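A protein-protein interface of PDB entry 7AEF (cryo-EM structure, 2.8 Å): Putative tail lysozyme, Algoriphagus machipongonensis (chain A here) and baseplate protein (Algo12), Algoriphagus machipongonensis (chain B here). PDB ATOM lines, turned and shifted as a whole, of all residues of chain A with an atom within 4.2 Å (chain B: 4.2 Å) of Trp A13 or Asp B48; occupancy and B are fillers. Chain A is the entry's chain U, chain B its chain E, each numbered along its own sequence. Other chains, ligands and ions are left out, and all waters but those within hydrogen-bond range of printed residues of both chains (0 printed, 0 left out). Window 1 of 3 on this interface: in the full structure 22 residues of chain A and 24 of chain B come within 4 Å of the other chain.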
ATOM      1  N   GLY A  12      35.420 -17.829  -7.350  1.00  0.00           N
ATOM      2  CA  GLY A  12      34.277 -17.276  -6.627  1.00  0.00           C
ATOM      3  C   GLY A  12      33.019 -18.117  -6.741  1.00  0.00           C
ATOM      4  O   GLY A  12      33.046 -19.208  -7.280  1.00  0.00           O
ATOM      5  N   TRP A  13      31.901 -17.589  -6.241  1.00  0.00           N
ATOM      6  CA  TRP A  13      30.627 -18.313  -6.235  1.00  0.00           C
ATOM      7  C   TRP A  13      30.059 -18.444  -7.644  1.00  0.00           C
ATOM      8  O   TRP A  13      30.175 -17.519  -8.444  1.00  0.00           O
ATOM      9  CB  TRP A  13      29.601 -17.564  -5.388  1.00  0.00           C
ATOM     10  CG  TRP A  13      29.820 -17.520  -3.898  1.00  0.00           C
ATOM     11  CD1 TRP A  13      30.952 -17.137  -3.234  1.00  0.00           C
ATOM     12  CD2 TRP A  13      28.857 -17.833  -2.892  1.00  0.00           C
ATOM     13  NE1 TRP A  13      30.749 -17.210  -1.885  1.00  0.00           N
ATOM     14  CE2 TRP A  13      29.469 -17.636  -1.653  1.00  0.00           C
ATOM     15  CE3 TRP A  13      27.533 -18.274  -2.924  1.00  0.00           C
ATOM     16  CZ2 TRP A  13      28.810 -17.864  -0.464  1.00  0.00           C
ATOM     17  CZ3 TRP A  13      26.885 -18.494  -1.739  1.00  0.00           C
ATOM     18  CH2 TRP A  13      27.518 -18.292  -0.532  1.00  0.00           C
ATOM     19  N   GLY A  14      29.410 -19.572  -7.955  1.00  0.00           N
ATOM     20  CA  GLY A  14      28.733 -19.685  -9.246  1.00  0.00           C
ATOM     21  C   GLY A  14      27.537 -18.750  -9.284  1.00  0.00           C
ATOM     22  O   GLY A  14      26.964 -18.454  -8.250  1.00  0.00           O
ATOM     23  N   PHE A  15      27.116 -18.231 -10.452  1.00  0.00           N
ATOM     24  CA  PHE A  15      26.022 -17.255 -10.377  1.00  0.00           C
ATOM     25  C   PHE A  15      24.704 -17.829  -9.919  1.00  0.00           C
ATOM     26  O   PHE A  15      24.105 -17.234  -9.016  1.00  0.00           O
ATOM     27  CB  PHE A  15      25.815 -16.493 -11.684  1.00  0.00           C
ATOM     28  CG  PHE A  15      24.409 -15.926 -11.821  1.00  0.00           C
ATOM     29  CD1 PHE A  15      23.829 -15.106 -10.835  1.00  0.00           C
ATOM     30  CD2 PHE A  15      23.716 -16.079 -12.991  1.00  0.00           C
ATOM     31  CE1 PHE A  15      22.587 -14.648 -10.927  1.00  0.00           C
ATOM     32  CE2 PHE A  15      22.463 -15.531 -13.127  1.00  0.00           C
ATOM     33  CZ  PHE A  15      21.906 -14.812 -12.093  1.00  0.00           C
ATOM     34  N   VAL A  26      28.773 -25.035  -1.415  1.00  0.00           N
ATOM     35  CA  VAL A  26      28.201 -24.295  -2.533  1.00  0.00           C
ATOM     36  C   VAL A  26      29.224 -24.333  -3.653  1.00  0.00           C
ATOM     37  O   VAL A  26      30.429 -24.204  -3.409  1.00  0.00           O
ATOM     38  CB  VAL A  26      27.820 -22.845  -2.144  1.00  0.00           C
ATOM     39  CG1 VAL A  26      29.041 -21.990  -1.781  1.00  0.00           C
ATOM     40  CG2 VAL A  26      27.021 -22.178  -3.262  1.00  0.00           C
ATOM     41  N   LYS A  27      28.763 -24.578  -4.870  1.00  0.00           N
ATOM     42  CA  LYS A  27      29.675 -24.665  -6.000  1.00  0.00           C
ATOM     43  C   LYS A  27      30.308 -23.327  -6.346  1.00  0.00           C
ATOM     44  O   LYS A  27      29.668 -22.273  -6.302  1.00  0.00           O
ATOM     45  CB  LYS A  27      28.956 -25.174  -7.234  1.00  0.00           C
ATOM     46  CG  LYS A  27      28.519 -26.588  -7.154  1.00  0.00           C
ATOM     47  CD  LYS A  27      27.920 -27.007  -8.471  1.00  0.00           C
ATOM     48  CE  LYS A  27      27.393 -28.409  -8.395  1.00  0.00           C
ATOM     49  NZ  LYS A  27      26.779 -28.835  -9.667  1.00  0.00           N
ATOM     50  N   THR A  29      33.324 -21.316  -9.172  1.00  0.00           N
ATOM     51  CA  THR A  29      33.858 -21.192 -10.523  1.00  0.00           C
ATOM     52  C   THR A  29      35.236 -20.536 -10.486  1.00  0.00           C
ATOM     53  O   THR A  29      35.613 -19.897  -9.510  1.00  0.00           O
ATOM     54  CB  THR A  29      32.892 -20.382 -11.425  1.00  0.00           C
ATOM     55  OG1 THR A  29      32.659 -19.070 -10.877  1.00  0.00           O
ATOM     56  CG2 THR A  29      31.574 -21.100 -11.558  1.00  0.00           C
ATOM     57  N   TRP B  41      38.295 -18.514  -1.577  1.00  0.00           N
ATOM     58  CA  TRP B  41      37.543 -17.408  -2.135  1.00  0.00           C
ATOM     59  C   TRP B  41      38.454 -16.203  -2.269  1.00  0.00           C
ATOM     60  O   TRP B  41      38.727 -15.522  -1.282  1.00  0.00           O
ATOM     61  CB  TRP B  41      36.357 -17.107  -1.240  1.00  0.00           C
ATOM     62  CG  TRP B  41      35.441 -16.043  -1.688  1.00  0.00           C
ATOM     63  CD1 TRP B  41      35.350 -15.469  -2.903  1.00  0.00           C
ATOM     64  CD2 TRP B  41      34.442 -15.441  -0.897  1.00  0.00           C
ATOM     65  NE1 TRP B  41      34.370 -14.540  -2.909  1.00  0.00           N
ATOM     66  CE2 TRP B  41      33.805 -14.501  -1.680  1.00  0.00           C
ATOM     67  CE3 TRP B  41      34.025 -15.611   0.409  1.00  0.00           C
ATOM     68  CZ2 TRP B  41      32.798 -13.735  -1.218  1.00  0.00           C
ATOM     69  CZ3 TRP B  41      33.005 -14.845   0.869  1.00  0.00           C
ATOM     70  CH2 TRP B  41      32.406 -13.922   0.066  1.00  0.00           C
ATOM     71  N   ASP B  43      38.201 -13.989  -5.419  1.00  0.00           N
ATOM     72  CA  ASP B  43      37.625 -13.039  -6.355  1.00  0.00           C
ATOM     73  C   ASP B  43      36.678 -12.124  -5.587  1.00  0.00           C
ATOM     74  O   ASP B  43      35.560 -12.526  -5.302  1.00  0.00           O
ATOM     75  CB  ASP B  43      36.900 -13.864  -7.413  1.00  0.00           C
ATOM     76  CG  ASP B  43      36.078 -13.058  -8.373  1.00  0.00           C
ATOM     77  OD1 ASP B  43      35.871 -11.864  -8.223  1.00  0.00           O
ATOM     78  OD2 ASP B  43      35.577 -13.637  -9.336  1.00  0.00           O
ATOM     79  N   ASN B  45      35.441  -9.143  -6.785  1.00  0.00           N
ATOM     80  CA  ASN B  45      34.858  -8.198  -7.719  1.00  0.00           C
ATOM     81  C   ASN B  45      33.359  -8.068  -7.519  1.00  0.00           C
ATOM     82  O   ASN B  45      32.704  -8.935  -6.954  1.00  0.00           O
ATOM     83  CB  ASN B  45      35.141  -8.631  -9.133  1.00  0.00           C
ATOM     84  CG  ASN B  45      36.509  -8.356  -9.520  1.00  0.00           C
ATOM     85  OD1 ASN B  45      36.889  -7.205  -9.667  1.00  0.00           O
ATOM     86  ND2 ASN B  45      37.284  -9.390  -9.678  1.00  0.00           N
ATOM     87  N   THR B  46      32.805  -6.986  -8.049  1.00  0.00           N
ATOM     88  CA  THR B  46      31.406  -6.652  -7.815  1.00  0.00           C
ATOM     89  C   THR B  46      30.392  -7.570  -8.497  1.00  0.00           C
ATOM     90  O   THR B  46      29.216  -7.518  -8.138  1.00  0.00           O
ATOM     91  CB  THR B  46      31.127  -5.232  -8.275  1.00  0.00           C
ATOM     92  OG1 THR B  46      31.539  -5.080  -9.631  1.00  0.00           O
ATOM     93  CG2 THR B  46      31.937  -4.284  -7.427  1.00  0.00           C
ATOM     94  N   HIS B  47      30.778  -8.399  -9.448  1.00  0.00           N
ATOM     95  CA  HIS B  47      29.798  -9.302 -10.031  1.00  0.00           C
ATOM     96  C   HIS B  47      29.587 -10.545  -9.181  1.00  0.00           C
ATOM     97  O   HIS B  47      28.720 -11.359  -9.504  1.00  0.00           O
ATOM     98  CB  HIS B  47      30.238  -9.757 -11.400  1.00  0.00           C
ATOM     99  CG  HIS B  47      31.409 -10.635 -11.333  1.00  0.00           C
ATOM    100  ND1 HIS B  47      32.667 -10.153 -11.106  1.00  0.00           N
ATOM    101  CD2 HIS B  47      31.513 -11.974 -11.399  1.00  0.00           C
ATOM    102  CE1 HIS B  47      33.509 -11.165 -11.057  1.00  0.00           C
ATOM    103  NE2 HIS B  47      32.832 -12.280 -11.229  1.00  0.00           N
ATOM    104  N   ASP B  48      30.393 -10.725  -8.145  1.00  0.00           N
ATOM    105  CA  ASP B  48      30.386 -11.914  -7.298  1.00  0.00           C
ATOM    106  C   ASP B  48      29.168 -11.958  -6.375  1.00  0.00           C
ATOM    107  O   ASP B  48      28.967 -11.026  -5.601  1.00  0.00           O
ATOM    108  CB  ASP B  48      31.668 -11.960  -6.468  1.00  0.00           C
ATOM    109  CG  ASP B  48      31.762 -13.202  -5.589  1.00  0.00           C
ATOM    110  OD1 ASP B  48      30.869 -14.025  -5.558  1.00  0.00           O
ATOM    111  OD2 ASP B  48      32.736 -13.354  -4.883  1.00  0.00           O
ATOM    112  N   PRO B  49      28.349 -13.026  -6.440  1.00  0.00           N
ATOM    113  CA  PRO B  49      27.217 -13.239  -5.528  1.00  0.00           C
ATOM    114  C   PRO B  49      27.582 -13.136  -4.062  1.00  0.00           C
ATOM    115  O   PRO B  49      26.779 -12.647  -3.268  1.00  0.00           O
ATOM    116  CB  PRO B  49      26.786 -14.663  -5.893  1.00  0.00           C
ATOM    117  CG  PRO B  49      27.169 -14.801  -7.322  1.00  0.00           C
ATOM    118  CD  PRO B  49      28.440 -14.061  -7.476  1.00  0.00           C
ATOM    119  N   GLY B  50      28.797 -13.551  -3.705  1.00  0.00           N
ATOM    120  CA  GLY B  50      29.256 -13.468  -2.332  1.00  0.00           C
ATOM    121  C   GLY B  50      29.280 -12.045  -1.833  1.00  0.00           C
ATOM    122  O   GLY B  50      28.703 -11.723  -0.793  1.00  0.00           O
ATOM    123  N   ILE B  51      29.949 -11.185  -2.591  1.00  0.00           N
ATOM    124  CA  ILE B  51      30.055  -9.775  -2.266  1.00  0.00           C
ATOM    125  C   ILE B  51      28.686  -9.118  -2.295  1.00  0.00           C
ATOM    126  O   ILE B  51      28.401  -8.248  -1.468  1.00  0.00           O
ATOM    127  CB  ILE B  51      31.048  -9.078  -3.220  1.00  0.00           C
ATOM    128  CG1 ILE B  51      32.472  -9.671  -3.071  1.00  0.00           C
ATOM    129  CG2 ILE B  51      31.056  -7.556  -3.006  1.00  0.00           C
ATOM    130  CD1 ILE B  51      33.132  -9.581  -1.687  1.00  0.00           C
ATOM    131  N   THR B  52      27.829  -9.504  -3.248  1.00  0.00           N
ATOM    132  CA  THR B  52      26.480  -8.949  -3.302  1.00  0.00           C
ATOM    133  C   THR B  52      25.731  -9.195  -1.996  1.00  0.00           C
ATOM    134  O   THR B  52      25.125  -8.276  -1.440  1.00  0.00           O
ATOM    135  CB  THR B  52      25.693  -9.548  -4.476  1.00  0.00           C
ATOM    136  OG1 THR B  52      26.327  -9.209  -5.711  1.00  0.00           O
ATOM    137  CG2 THR B  52      24.261  -9.034  -4.494  1.00  0.00           C
ATOM    138  N   TYR B 425      18.772 -20.972   2.104  1.00  0.00           N
ATOM    139  CA  TYR B 425      20.015 -20.475   2.675  1.00  0.00           C
ATOM    140  C   TYR B 425      19.836 -19.109   3.315  1.00  0.00           C
ATOM    141  O   TYR B 425      20.245 -18.895   4.456  1.00  0.00           O
ATOM    142  CB  TYR B 425      21.074 -20.419   1.589  1.00  0.00           C
ATOM    143  CG  TYR B 425      22.391 -19.856   2.004  1.00  0.00           C
ATOM    144  CD1 TYR B 425      23.255 -20.596   2.770  1.00  0.00           C
ATOM    145  CD2 TYR B 425      22.780 -18.600   1.588  1.00  0.00           C
ATOM    146  CE1 TYR B 425      24.466 -20.099   3.125  1.00  0.00           C
ATOM    147  CE2 TYR B 425      23.993 -18.100   1.937  1.00  0.00           C
ATOM    148  CZ  TYR B 425      24.834 -18.854   2.707  1.00  0.00           C
ATOM    149  OH  TYR B 425      26.054 -18.356   3.065  1.00  0.00           O
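The indole nitrogen of Trp B41 lies within hydrogen-bond range of the side-chain carboxylate of Asp B48, 2.8 Å away. OD1 of Asp B48 sits at hydrogen-bond distance from N of Gly B50 (2.8 Å). OG1 of Thr B52 lies within hydrogen-bond range of O of Asp B48, at 3.2 Å. O of Lys A27 lies within hydrogen-bond range of N of Gly A14.
Trp A13 touches Asp B48 (CB to OD1, 3.8 Å). O of Trp A13 touches CD of Pro B49, 3.99 Å away. Tyr B425 touches Trp A13 (OH to CH2, 3.9 Å). Gly A14 touches Pro B49.
Of the printed residues of chain B, Trp A13 touches Asp B48 (3.8 Å), Pro B49 (3.99 Å) and Tyr B425 (3.9 Å). Of the printed residues of chain B, Gly A14 touches Pro B49 (3.8 Å). Asp B48 touches just one residue of chain A: Trp A13. Printed residues of chain A within 4 Å of Pro B49: Trp A13 (3.99 Å) and Gly A14 (3.8 Å). Printed residues of chain A within 4 Å of Tyr B425: Trp A13 (3.9 Å). The nearest printed residue of chain B that does not touch Trp A13 is Gly B50 (4.1 Å). The nearest printed residue of chain A that does not touch Asp B48 is Gly A12 (4.6 Å).
Of the 7 printed residues of chain A, 2 touch a printed residue of chain B. Hydrophobic or aromatic side chains of chain A within 4 Å of the printed part of chain B: Trp A13. Of the 11 printed residues of chain B, 3 touch a printed residue of chain A. Printed residues of chain B that touch a printed residue of chain A: Asp B48, Pro B49 and Tyr B425. Hydrophobic or aromatic side chains of chain B that line the printed part of chain A: Pro B49 and Tyr B425.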
